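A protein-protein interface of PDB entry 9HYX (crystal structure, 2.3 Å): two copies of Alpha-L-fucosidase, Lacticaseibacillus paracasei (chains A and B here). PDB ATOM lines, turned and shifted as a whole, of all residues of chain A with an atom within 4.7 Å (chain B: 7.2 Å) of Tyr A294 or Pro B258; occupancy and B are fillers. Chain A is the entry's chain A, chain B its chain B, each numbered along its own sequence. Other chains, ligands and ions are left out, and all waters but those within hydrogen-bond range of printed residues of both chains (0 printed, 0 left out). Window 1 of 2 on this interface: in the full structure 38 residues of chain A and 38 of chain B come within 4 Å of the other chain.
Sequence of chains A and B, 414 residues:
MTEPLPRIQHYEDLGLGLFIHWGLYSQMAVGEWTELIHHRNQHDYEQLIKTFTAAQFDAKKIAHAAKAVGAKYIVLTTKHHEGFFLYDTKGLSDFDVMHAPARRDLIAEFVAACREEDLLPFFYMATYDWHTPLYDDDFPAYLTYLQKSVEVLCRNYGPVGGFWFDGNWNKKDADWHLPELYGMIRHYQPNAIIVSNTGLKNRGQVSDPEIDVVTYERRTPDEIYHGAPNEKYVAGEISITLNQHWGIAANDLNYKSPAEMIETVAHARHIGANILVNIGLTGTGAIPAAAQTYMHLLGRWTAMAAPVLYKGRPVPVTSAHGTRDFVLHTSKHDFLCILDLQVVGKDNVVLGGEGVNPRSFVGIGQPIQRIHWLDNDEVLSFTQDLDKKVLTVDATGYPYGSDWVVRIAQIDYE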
ATOM      1  N   LEU A 242      -8.933  19.292  10.032  1.00  0.00           N
ATOM      2  CA  LEU A 242     -10.079  18.633   9.418  1.00  0.00           C
ATOM      3  C   LEU A 242     -10.579  19.371   8.171  1.00  0.00           C
ATOM      4  O   LEU A 242     -11.021  18.711   7.224  1.00  0.00           O
ATOM      5  CB  LEU A 242     -11.201  18.483  10.436  1.00  0.00           C
ATOM      6  CG  LEU A 242     -10.824  17.663  11.675  1.00  0.00           C
ATOM      7  CD1 LEU A 242     -11.983  17.677  12.648  1.00  0.00           C
ATOM      8  CD2 LEU A 242     -10.354  16.263  11.352  1.00  0.00           C
ATOM      9  N   LEU A 253     -16.282  24.768   4.542  1.00  0.00           N
ATOM     10  CA  LEU A 253     -17.052  23.549   4.342  1.00  0.00           C
ATOM     11  C   LEU A 253     -16.157  22.461   3.764  1.00  0.00           C
ATOM     12  O   LEU A 253     -16.612  21.340   3.519  1.00  0.00           O
ATOM     13  CB  LEU A 253     -18.202  23.813   3.377  1.00  0.00           C
ATOM     14  CG  LEU A 253     -19.073  25.016   3.731  1.00  0.00           C
ATOM     15  CD1 LEU A 253     -20.261  25.105   2.763  1.00  0.00           C
ATOM     16  CD2 LEU A 253     -19.481  25.053   5.211  1.00  0.00           C
ATOM     17  N   TYR A 255     -14.149  20.107   4.365  1.00  0.00           N
ATOM     18  CA  TYR A 255     -13.640  19.066   5.250  1.00  0.00           C
ATOM     19  C   TYR A 255     -13.124  17.887   4.435  1.00  0.00           C
ATOM     20  O   TYR A 255     -13.702  17.539   3.400  1.00  0.00           O
ATOM     21  CB  TYR A 255     -14.827  18.607   6.090  1.00  0.00           C
ATOM     22  CG  TYR A 255     -15.037  19.490   7.314  1.00  0.00           C
ATOM     23  CD1 TYR A 255     -15.673  20.721   7.197  1.00  0.00           C
ATOM     24  CD2 TYR A 255     -14.578  19.093   8.579  1.00  0.00           C
ATOM     25  CE1 TYR A 255     -15.875  21.531   8.308  1.00  0.00           C
ATOM     26  CE2 TYR A 255     -14.758  19.909   9.689  1.00  0.00           C
ATOM     27  CZ  TYR A 255     -15.412  21.126   9.541  1.00  0.00           C
ATOM     28  OH  TYR A 255     -15.622  21.962  10.587  1.00  0.00           O
ATOM     29  N   LYS A 256     -12.037  17.276   4.926  1.00  0.00           N
ATOM     30  CA  LYS A 256     -11.498  16.035   4.393  1.00  0.00           C
ATOM     31  C   LYS A 256     -12.429  14.892   4.792  1.00  0.00           C
ATOM     32  O   LYS A 256     -13.171  15.004   5.775  1.00  0.00           O
ATOM     33  CB  LYS A 256     -10.146  15.817   5.071  1.00  0.00           C
ATOM     34  CG  LYS A 256      -9.165  16.937   4.775  1.00  0.00           C
ATOM     35  CD  LYS A 256      -7.813  16.779   5.475  1.00  0.00           C
ATOM     36  CE  LYS A 256      -6.902  17.962   5.177  1.00  0.00           C
ATOM     37  NZ  LYS A 256      -7.558  19.258   5.458  1.00  0.00           N
ATOM     38  N   SER A 257     -12.396  13.787   4.041  1.00  0.00           N
ATOM     39  CA  SER A 257     -13.193  12.647   4.450  1.00  0.00           C
ATOM     40  C   SER A 257     -12.594  12.013   5.702  1.00  0.00           C
ATOM     41  O   SER A 257     -11.376  12.019   5.901  1.00  0.00           O
ATOM     42  CB  SER A 257     -13.315  11.614   3.358  1.00  0.00           C
ATOM     43  OG  SER A 257     -12.064  11.007   3.129  1.00  0.00           O
ATOM     44  N   PRO A 258     -13.453  11.428   6.565  1.00  0.00           N
ATOM     45  CA  PRO A 258     -12.984  10.527   7.607  1.00  0.00           C
ATOM     46  C   PRO A 258     -12.018   9.461   7.075  1.00  0.00           C
ATOM     47  O   PRO A 258     -11.039   9.127   7.739  1.00  0.00           O
ATOM     48  CB  PRO A 258     -14.297  10.045   8.259  1.00  0.00           C
ATOM     49  CG  PRO A 258     -15.208  11.271   8.034  1.00  0.00           C
ATOM     50  CD  PRO A 258     -14.909  11.674   6.625  1.00  0.00           C
ATOM     51  N   MET A 261      -8.599  10.876   6.761  1.00  0.00           N
ATOM     52  CA  MET A 261      -8.065  11.045   8.100  1.00  0.00           C
ATOM     53  C   MET A 261      -7.454   9.732   8.599  1.00  0.00           C
ATOM     54  O   MET A 261      -6.310   9.713   9.069  1.00  0.00           O
ATOM     55  CB  MET A 261      -9.155  11.543   9.054  1.00  0.00           C
ATOM     56  CG  MET A 261      -8.706  11.640  10.485  1.00  0.00           C
ATOM     57  SD  MET A 261     -10.105  11.966  11.598  1.00  0.00           S
ATOM     58  CE  MET A 261     -11.275  10.618  11.286  1.00  0.00           C
ATOM     59  N   ALA A 290     -18.877  19.149  14.654  1.00  0.00           N
ATOM     60  CA  ALA A 290     -18.202  18.528  13.509  1.00  0.00           C
ATOM     61  C   ALA A 290     -16.955  17.760  13.952  1.00  0.00           C
ATOM     62  O   ALA A 290     -16.717  16.647  13.508  1.00  0.00           O
ATOM     63  CB  ALA A 290     -17.895  19.531  12.395  1.00  0.00           C
ATOM     64  N   ALA A 291     -16.176  18.350  14.877  1.00  0.00           N
ATOM     65  CA  ALA A 291     -14.977  17.703  15.369  1.00  0.00           C
ATOM     66  C   ALA A 291     -15.304  16.414  16.131  1.00  0.00           C
ATOM     67  O   ALA A 291     -14.600  15.430  15.966  1.00  0.00           O
ATOM     68  CB  ALA A 291     -14.149  18.670  16.185  1.00  0.00           C
ATOM     69  N   GLN A 292     -16.355  16.434  16.967  1.00  0.00           N
ATOM     70  CA  GLN A 292     -16.837  15.251  17.665  1.00  0.00           C
ATOM     71  C   GLN A 292     -17.094  14.096  16.685  1.00  0.00           C
ATOM     72  O   GLN A 292     -16.716  12.964  16.963  1.00  0.00           O
ATOM     73  CB  GLN A 292     -18.081  15.516  18.523  1.00  0.00           C
ATOM     74  CG  GLN A 292     -17.793  16.289  19.810  1.00  0.00           C
ATOM     75  CD  GLN A 292     -19.002  16.740  20.610  1.00  0.00           C
ATOM     76  OE1 GLN A 292     -19.197  17.939  20.872  1.00  0.00           O
ATOM     77  NE2 GLN A 292     -19.797  15.772  21.051  1.00  0.00           N
ATOM     78  N   THR A 293     -17.733  14.371  15.539  1.00  0.00           N
ATOM     79  CA  THR A 293     -18.035  13.326  14.561  1.00  0.00           C
ATOM     80  C   THR A 293     -16.743  12.664  14.091  1.00  0.00           C
ATOM     81  O   THR A 293     -16.662  11.455  14.025  1.00  0.00           O
ATOM     82  CB  THR A 293     -18.813  13.906  13.367  1.00  0.00           C
ATOM     83  OG1 THR A 293     -20.117  14.167  13.892  1.00  0.00           O
ATOM     84  CG2 THR A 293     -18.857  12.989  12.154  1.00  0.00           C
ATOM     85  N   TYR A 294     -15.725  13.459  13.768  1.00  0.00           N
ATOM     86  CA  TYR A 294     -14.467  12.924  13.269  1.00  0.00           C
ATOM     87  C   TYR A 294     -13.757  12.133  14.370  1.00  0.00           C
ATOM     88  O   TYR A 294     -13.149  11.086  14.086  1.00  0.00           O
ATOM     89  CB  TYR A 294     -13.595  14.073  12.744  1.00  0.00           C
ATOM     90  CG  TYR A 294     -13.974  14.425  11.317  1.00  0.00           C
ATOM     91  CD1 TYR A 294     -15.132  15.135  11.053  1.00  0.00           C
ATOM     92  CD2 TYR A 294     -13.186  14.026  10.230  1.00  0.00           C
ATOM     93  CE1 TYR A 294     -15.496  15.466   9.759  1.00  0.00           C
ATOM     94  CE2 TYR A 294     -13.531  14.349   8.930  1.00  0.00           C
ATOM     95  CZ  TYR A 294     -14.682  15.086   8.701  1.00  0.00           C
ATOM     96  OH  TYR A 294     -15.073  15.404   7.422  1.00  0.00           O
ATOM     97  N   MET A 295     -13.858  12.628  15.618  1.00  0.00           N
ATOM     98  CA  MET A 295     -13.206  11.945  16.721  1.00  0.00           C
ATOM     99  C   MET A 295     -13.863  10.591  16.975  1.00  0.00           C
ATOM    100  O   MET A 295     -13.170   9.623  17.283  1.00  0.00           O
ATOM    101  CB  MET A 295     -13.170  12.838  17.972  1.00  0.00           C
ATOM    102  CG  MET A 295     -12.101  13.954  17.855  1.00  0.00           C
ATOM    103  SD  MET A 295     -12.360  15.235  19.129  1.00  0.00           S
ATOM    104  CE  MET A 295     -11.585  14.237  20.421  1.00  0.00           C
ATOM    105  N   HIS A 296     -15.198  10.522  16.876  1.00  0.00           N
ATOM    106  CA  HIS A 296     -15.899   9.265  17.088  1.00  0.00           C
ATOM    107  C   HIS A 296     -15.478   8.256  16.012  1.00  0.00           C
ATOM    108  O   HIS A 296     -15.204   7.096  16.340  1.00  0.00           O
ATOM    109  CB  HIS A 296     -17.414   9.446  17.196  1.00  0.00           C
ATOM    110  CG  HIS A 296     -17.812  10.097  18.486  1.00  0.00           C
ATOM    111  ND1 HIS A 296     -18.813  11.050  18.601  1.00  0.00           N
ATOM    112  CD2 HIS A 296     -17.305   9.973  19.723  1.00  0.00           C
ATOM    113  CE1 HIS A 296     -18.909  11.464  19.858  1.00  0.00           C
ATOM    114  NE2 HIS A 296     -18.018  10.814  20.560  1.00  0.00           N
ATOM    115  N   LEU A 297     -15.384   8.700  14.748  1.00  0.00           N
ATOM    116  CA  LEU A 297     -15.010   7.765  13.696  1.00  0.00           C
ATOM    117  C   LEU A 297     -13.568   7.308  13.884  1.00  0.00           C
ATOM    118  O   LEU A 297     -13.297   6.113  13.827  1.00  0.00           O
ATOM    119  CB  LEU A 297     -15.247   8.371  12.319  1.00  0.00           C
ATOM    120  CG  LEU A 297     -16.728   8.670  12.025  1.00  0.00           C
ATOM    121  CD1 LEU A 297     -16.863   9.486  10.751  1.00  0.00           C
ATOM    122  CD2 LEU A 297     -17.578   7.411  11.899  1.00  0.00           C
ATOM    123  N   LEU A 298     -12.652   8.222  14.146  1.00  0.00           N
ATOM    124  CA  LEU A 298     -11.258   7.892  14.349  1.00  0.00           C
ATOM    125  C   LEU A 298     -11.056   6.983  15.552  1.00  0.00           C
ATOM    126  O   LEU A 298     -10.253   6.103  15.524  1.00  0.00           O
ATOM    127  CB  LEU A 298     -10.413   9.158  14.461  1.00  0.00           C
ATOM    128  CG  LEU A 298      -8.929   8.971  14.721  1.00  0.00           C
ATOM    129  CD1 LEU A 298      -8.264   8.152  13.647  1.00  0.00           C
ATOM    130  CD2 LEU A 298      -8.224  10.290  14.898  1.00  0.00           C
ATOM    131  N   TYR B 255     -16.705   7.176   5.348  1.00  0.00           N
ATOM    132  CA  TYR B 255     -17.510   8.324   4.967  1.00  0.00           C
ATOM    133  C   TYR B 255     -16.833   9.124   3.850  1.00  0.00           C
ATOM    134  O   TYR B 255     -15.610   9.260   3.829  1.00  0.00           O
ATOM    135  CB  TYR B 255     -17.615   9.194   6.224  1.00  0.00           C
ATOM    136  CG  TYR B 255     -18.744   8.735   7.131  1.00  0.00           C
ATOM    137  CD1 TYR B 255     -18.584   7.626   7.970  1.00  0.00           C
ATOM    138  CD2 TYR B 255     -19.985   9.376   7.123  1.00  0.00           C
ATOM    139  CE1 TYR B 255     -19.603   7.209   8.810  1.00  0.00           C
ATOM    140  CE2 TYR B 255     -21.016   8.964   7.959  1.00  0.00           C
ATOM    141  CZ  TYR B 255     -20.817   7.880   8.796  1.00  0.00           C
ATOM    142  OH  TYR B 255     -21.797   7.447   9.619  1.00  0.00           O
ATOM    143  N   LYS B 256     -17.652   9.663   2.945  1.00  0.00           N
ATOM    144  CA  LYS B 256     -17.236  10.601   1.910  1.00  0.00           C
ATOM    145  C   LYS B 256     -16.949  11.950   2.570  1.00  0.00           C
ATOM    146  O   LYS B 256     -17.461  12.239   3.655  1.00  0.00           O
ATOM    147  CB  LYS B 256     -18.420  10.768   0.952  1.00  0.00           C
ATOM    148  CG  LYS B 256     -18.786   9.452   0.276  1.00  0.00           C
ATOM    149  CD  LYS B 256     -19.968   9.542  -0.680  1.00  0.00           C
ATOM    150  CE  LYS B 256     -20.369   8.212  -1.265  1.00  0.00           C
ATOM    151  NZ  LYS B 256     -20.549   7.178  -0.227  1.00  0.00           N
ATOM    152  N   SER B 257     -16.117  12.776   1.927  1.00  0.00           N
ATOM    153  CA  SER B 257     -15.908  14.103   2.482  1.00  0.00           C
ATOM    154  C   SER B 257     -17.155  14.963   2.318  1.00  0.00           C
ATOM    155  O   SER B 257     -17.905  14.806   1.369  1.00  0.00           O
ATOM    156  CB  SER B 257     -14.725  14.794   1.863  1.00  0.00           C
ATOM    157  OG  SER B 257     -15.002  15.093   0.516  1.00  0.00           O
ATOM    158  N   PRO B 258     -17.414  15.889   3.261  1.00  0.00           N
ATOM    159  CA  PRO B 258     -18.400  16.940   3.036  1.00  0.00           C
ATOM    160  C   PRO B 258     -18.203  17.668   1.697  1.00  0.00           C
ATOM    161  O   PRO B 258     -19.185  18.014   1.027  1.00  0.00           O
ATOM    162  CB  PRO B 258     -18.311  17.783   4.324  1.00  0.00           C
ATOM    163  CG  PRO B 258     -17.855  16.739   5.362  1.00  0.00           C
ATOM    164  CD  PRO B 258     -16.833  15.903   4.617  1.00  0.00           C
ATOM    165  N   ALA B 259     -16.952  17.838   1.261  1.00  0.00           N
ATOM    166  CA  ALA B 259     -16.676  18.498  -0.008  1.00  0.00           C
ATOM    167  C   ALA B 259     -17.281  17.688  -1.155  1.00  0.00           C
ATOM    168  O   ALA B 259     -17.872  18.246  -2.078  1.00  0.00           O
ATOM    169  CB  ALA B 259     -15.158  18.667  -0.229  1.00  0.00           C
ATOM    170  N   GLU B 260     -17.073  16.375  -1.145  1.00  0.00           N
ATOM    171  CA  GLU B 260     -17.625  15.527  -2.194  1.00  0.00           C
ATOM    172  C   GLU B 260     -19.164  15.594  -2.179  1.00  0.00           C
ATOM    173  O   GLU B 260     -19.798  15.611  -3.232  1.00  0.00           O
ATOM    174  CB  GLU B 260     -17.116  14.094  -2.037  1.00  0.00           C
ATOM    175  CG  GLU B 260     -17.811  13.134  -2.990  1.00  0.00           C
ATOM    176  CD  GLU B 260     -17.271  11.706  -2.982  1.00  0.00           C
ATOM    177  OE1 GLU B 260     -16.280  11.398  -2.240  1.00  0.00           O
ATOM    178  OE2 GLU B 260     -17.862  10.875  -3.713  1.00  0.00           O
ATOM    179  N   MET B 261     -19.763  15.653  -0.988  1.00  0.00           N
ATOM    180  CA  MET B 261     -21.204  15.790  -0.862  1.00  0.00           C
ATOM    181  C   MET B 261     -21.697  17.067  -1.568  1.00  0.00           C
ATOM    182  O   MET B 261     -22.629  17.007  -2.379  1.00  0.00           O
ATOM    183  CB  MET B 261     -21.596  15.762   0.617  1.00  0.00           C
ATOM    184  CG  MET B 261     -23.070  16.015   0.828  1.00  0.00           C
ATOM    185  SD  MET B 261     -23.502  16.251   2.560  1.00  0.00           S
ATOM    186  CE  MET B 261     -22.416  17.604   3.067  1.00  0.00           C
ATOM    187  N   ILE B 262     -21.040  18.203  -1.295  1.00  0.00           N
ATOM    188  CA  ILE B 262     -21.410  19.460  -1.930  1.00  0.00           C
ATOM    189  C   ILE B 262     -21.207  19.371  -3.442  1.00  0.00           C
ATOM    190  O   ILE B 262     -22.084  19.789  -4.205  1.00  0.00           O
ATOM    191  CB  ILE B 262     -20.635  20.642  -1.314  1.00  0.00           C
ATOM    192  CG1 ILE B 262     -21.178  20.942   0.071  1.00  0.00           C
ATOM    193  CG2 ILE B 262     -20.716  21.882  -2.204  1.00  0.00           C
ATOM    194  CD1 ILE B 262     -20.199  21.714   0.953  1.00  0.00           C
ATOM    195  N   GLU B 263     -20.067  18.821  -3.875  1.00  0.00           N
ATOM    196  CA  GLU B 263     -19.838  18.662  -5.313  1.00  0.00           C
ATOM    197  C   GLU B 263     -20.919  17.788  -5.955  1.00  0.00           C
ATOM    198  O   GLU B 263     -21.285  18.027  -7.103  1.00  0.00           O
ATOM    199  CB  GLU B 263     -18.453  18.124  -5.684  1.00  0.00           C
ATOM    200  CG  GLU B 263     -17.318  19.093  -5.330  1.00  0.00           C
ATOM    201  CD  GLU B 263     -15.909  18.778  -5.827  1.00  0.00           C
ATOM    202  OE1 GLU B 263     -15.771  17.746  -6.518  1.00  0.00           O
ATOM    203  OE2 GLU B 263     -14.941  19.558  -5.619  1.00  0.00           O
ATOM    204  N   THR B 264     -21.422  16.770  -5.231  1.00  0.00           N
ATOM    205  CA  THR B 264     -22.400  15.854  -5.824  1.00  0.00           C
ATOM    206  C   THR B 264     -23.726  16.587  -6.009  1.00  0.00           C
ATOM    207  O   THR B 264     -24.385  16.442  -7.040  1.00  0.00           O
ATOM    208  CB  THR B 264     -22.559  14.580  -4.989  1.00  0.00           C
ATOM    209  OG1 THR B 264     -21.244  14.026  -4.967  1.00  0.00           O
ATOM    210  CG2 THR B 264     -23.457  13.550  -5.653  1.00  0.00           C
ATOM    211  N   ALA B 290     -23.325  11.784  13.388  1.00  0.00           N
ATOM    212  CA  ALA B 290     -22.511  11.927  12.187  1.00  0.00           C
ATOM    213  C   ALA B 290     -23.326  12.560  11.059  1.00  0.00           C
ATOM    214  O   ALA B 290     -22.837  13.456  10.372  1.00  0.00           O
ATOM    215  CB  ALA B 290     -21.880  10.586  11.799  1.00  0.00           C
ATOM    216  N   THR B 293     -23.778  16.344  11.360  1.00  0.00           N
ATOM    217  CA  THR B 293     -22.638  17.150  10.936  1.00  0.00           C
ATOM    218  C   THR B 293     -22.688  17.449   9.439  1.00  0.00           C
ATOM    219  O   THR B 293     -22.506  18.589   9.027  1.00  0.00           O
ATOM    220  CB  THR B 293     -21.296  16.479  11.309  1.00  0.00           C
ATOM    221  OG1 THR B 293     -21.119  16.523  12.730  1.00  0.00           O
ATOM    222  CG2 THR B 293     -20.133  17.185  10.640  1.00  0.00           C
ATOM    223  N   TYR B 294     -22.940  16.429   8.632  1.00  0.00           N
ATOM    224  CA  TYR B 294     -23.004  16.615   7.186  1.00  0.00           C
ATOM    225  C   TYR B 294     -24.159  17.522   6.782  1.00  0.00           C
ATOM    226  O   TYR B 294     -24.024  18.334   5.875  1.00  0.00           O
ATOM    227  CB  TYR B 294     -23.095  15.263   6.474  1.00  0.00           C
ATOM    228  CG  TYR B 294     -21.772  14.550   6.366  1.00  0.00           C
ATOM    229  CD1 TYR B 294     -21.229  13.888   7.455  1.00  0.00           C
ATOM    230  CD2 TYR B 294     -21.062  14.541   5.175  1.00  0.00           C
ATOM    231  CE1 TYR B 294     -20.017  13.237   7.362  1.00  0.00           C
ATOM    232  CE2 TYR B 294     -19.850  13.893   5.071  1.00  0.00           C
ATOM    233  CZ  TYR B 294     -19.332  13.243   6.170  1.00  0.00           C
ATOM    234  OH  TYR B 294     -18.126  12.596   6.077  1.00  0.00           O
ATOM    235  N   LEU B 297     -23.232  21.163   7.454  1.00  0.00           N
ATOM    236  CA  LEU B 297     -22.300  21.664   6.457  1.00  0.00           C
ATOM    237  C   LEU B 297     -23.012  21.855   5.135  1.00  0.00           C
ATOM    238  O   LEU B 297     -22.845  22.875   4.479  1.00  0.00           O
ATOM    239  CB  LEU B 297     -21.123  20.709   6.313  1.00  0.00           C
ATOM    240  CG  LEU B 297     -20.229  20.590   7.547  1.00  0.00           C
ATOM    241  CD1 LEU B 297     -19.196  19.489   7.374  1.00  0.00           C
ATOM    242  CD2 LEU B 297     -19.558  21.918   7.859  1.00  0.00           C
ATOM    243  N   LEU B 298     -23.816  20.878   4.750  1.00  0.00           N
ATOM    244  CA  LEU B 298     -24.578  20.979   3.519  1.00  0.00           C
ATOM    245  C   LEU B 298     -25.561  22.135   3.617  1.00  0.00           C
ATOM    246  O   LEU B 298     -25.783  22.848   2.656  1.00  0.00           O
ATOM    247  CB  LEU B 298     -25.311  19.672   3.224  1.00  0.00           C
ATOM    248  CG  LEU B 298     -26.109  19.614   1.923  1.00  0.00           C
ATOM    249  CD1 LEU B 298     -25.253  20.051   0.749  1.00  0.00           C
ATOM    250  CD2 LEU B 298     -26.666  18.221   1.697  1.00  0.00           C
ATOM    251  N   VAL B 405     -16.255  25.272  -1.494  1.00  0.00           N
ATOM    252  CA  VAL B 405     -16.104  24.061  -2.291  1.00  0.00           C
ATOM    253  C   VAL B 405     -16.610  24.301  -3.715  1.00  0.00           C
ATOM    254  O   VAL B 405     -15.863  24.082  -4.661  1.00  0.00           O
ATOM    255  CB  VAL B 405     -16.726  22.788  -1.674  1.00  0.00           C
ATOM    256  CG1 VAL B 405     -16.517  21.568  -2.566  1.00  0.00           C
ATOM    257  CG2 VAL B 405     -16.164  22.542  -0.269  1.00  0.00           C
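The side-chain hydroxyl (OG1) of Thr A293 is in hydrogen-bond range of the side-chain hydroxyl (OG1) of Thr B293, 2.8 Å away.
N of Lys A256 lies within hydrogen-bond range of O of Leu A242. The backbone carbonyl oxygen (O) of Lys A256 sits at hydrogen-bond distance from the side-chain hydroxyl (OH) of Tyr A294 (2.5 Å). OH of Tyr B294 sits at hydrogen-bond distance from O of Lys B256. The side-chain hydroxyl (OG) of Ser B257 lies close to the backbone NH (N) of Ala B259, at 3.4 Å. The side-chain hydroxyl (OG) of Ser B257 sits at hydrogen-bond distance from the backbone NH (N) of Glu B260 (2.9 Å).
Leu A253 touches Ile B262. Leu A253 touches Leu B297 (CD1 to O, 3.8 Å). CG2 of Val B405 touches O of Leu A253 (3.999 Å). Tyr A255 touches Ala B259. CE1 of Tyr A255 touches CD2 of Leu B297 (3.7 Å). Pro B258 touches Lys A256. Ser A257 touches Lys B256 (CB to C, 3.7 Å). Pro A258 touches Tyr B294. Pro B258 touches Tyr A294. Tyr B255 touches Leu A297.
Tyr A294 touches just one residue of chain B: Pro B258 (3.3 Å). Of chain A, only Tyr A255 (3.6 Å), Lys A256 (3.9 Å) and Tyr A294 (3.3 Å) come within 4 Å of Pro B258. Printed residues of chain B within 4 Å of Ser A257: Tyr B255, Lys B256 and Ser B257. Of the printed residues of chain A, Tyr B294 touches Pro A258. Of the printed residues of chain A, Leu B297 touches Leu A253 and Tyr A255. Glu B263 touches none of the printed residues of chain A. Gln A292 touches none of the printed residues of chain B. The nearest residue of chain B that does not touch Tyr A294 is Tyr B294 (4.4 Å). The nearest printed residue of chain A that does not touch Ile B262 is Tyr A255 (7.1 Å).
Hydrophobic or aromatic side chains of chain A that line the printed part of chain B: Leu A253, Tyr A255, Pro A258, Ala A290, Tyr A294 and Leu A297. Printed residues of chain B that touch a printed residue of chain A: Tyr B255, Lys B256, Ser B257, Pro B258, Ala B259, Ile B262, Ala B290, Thr B293, Tyr B294, Leu B297 and Val B405. Hydrophobic or aromatic side chains of chain B that line the printed part of chain A: Tyr B255, Pro B258, Ile B262, Ala B290, Tyr B294, Leu B297 and Val B405.
Tyr A255 touches Ser B257, and with the chains exchanged Ser A257 touches Tyr B255. Lys A256 touches Ser B257, and with the chains exchanged Ser A257 touches Lys B256. Ser B257 touches its own counterpart, Ser A257. Thr B293 touches its own counterpart, Thr A293. Of the 20 pairs that touch across the chains among the printed residues, 16 have their exchanged pair printed and touching as well.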
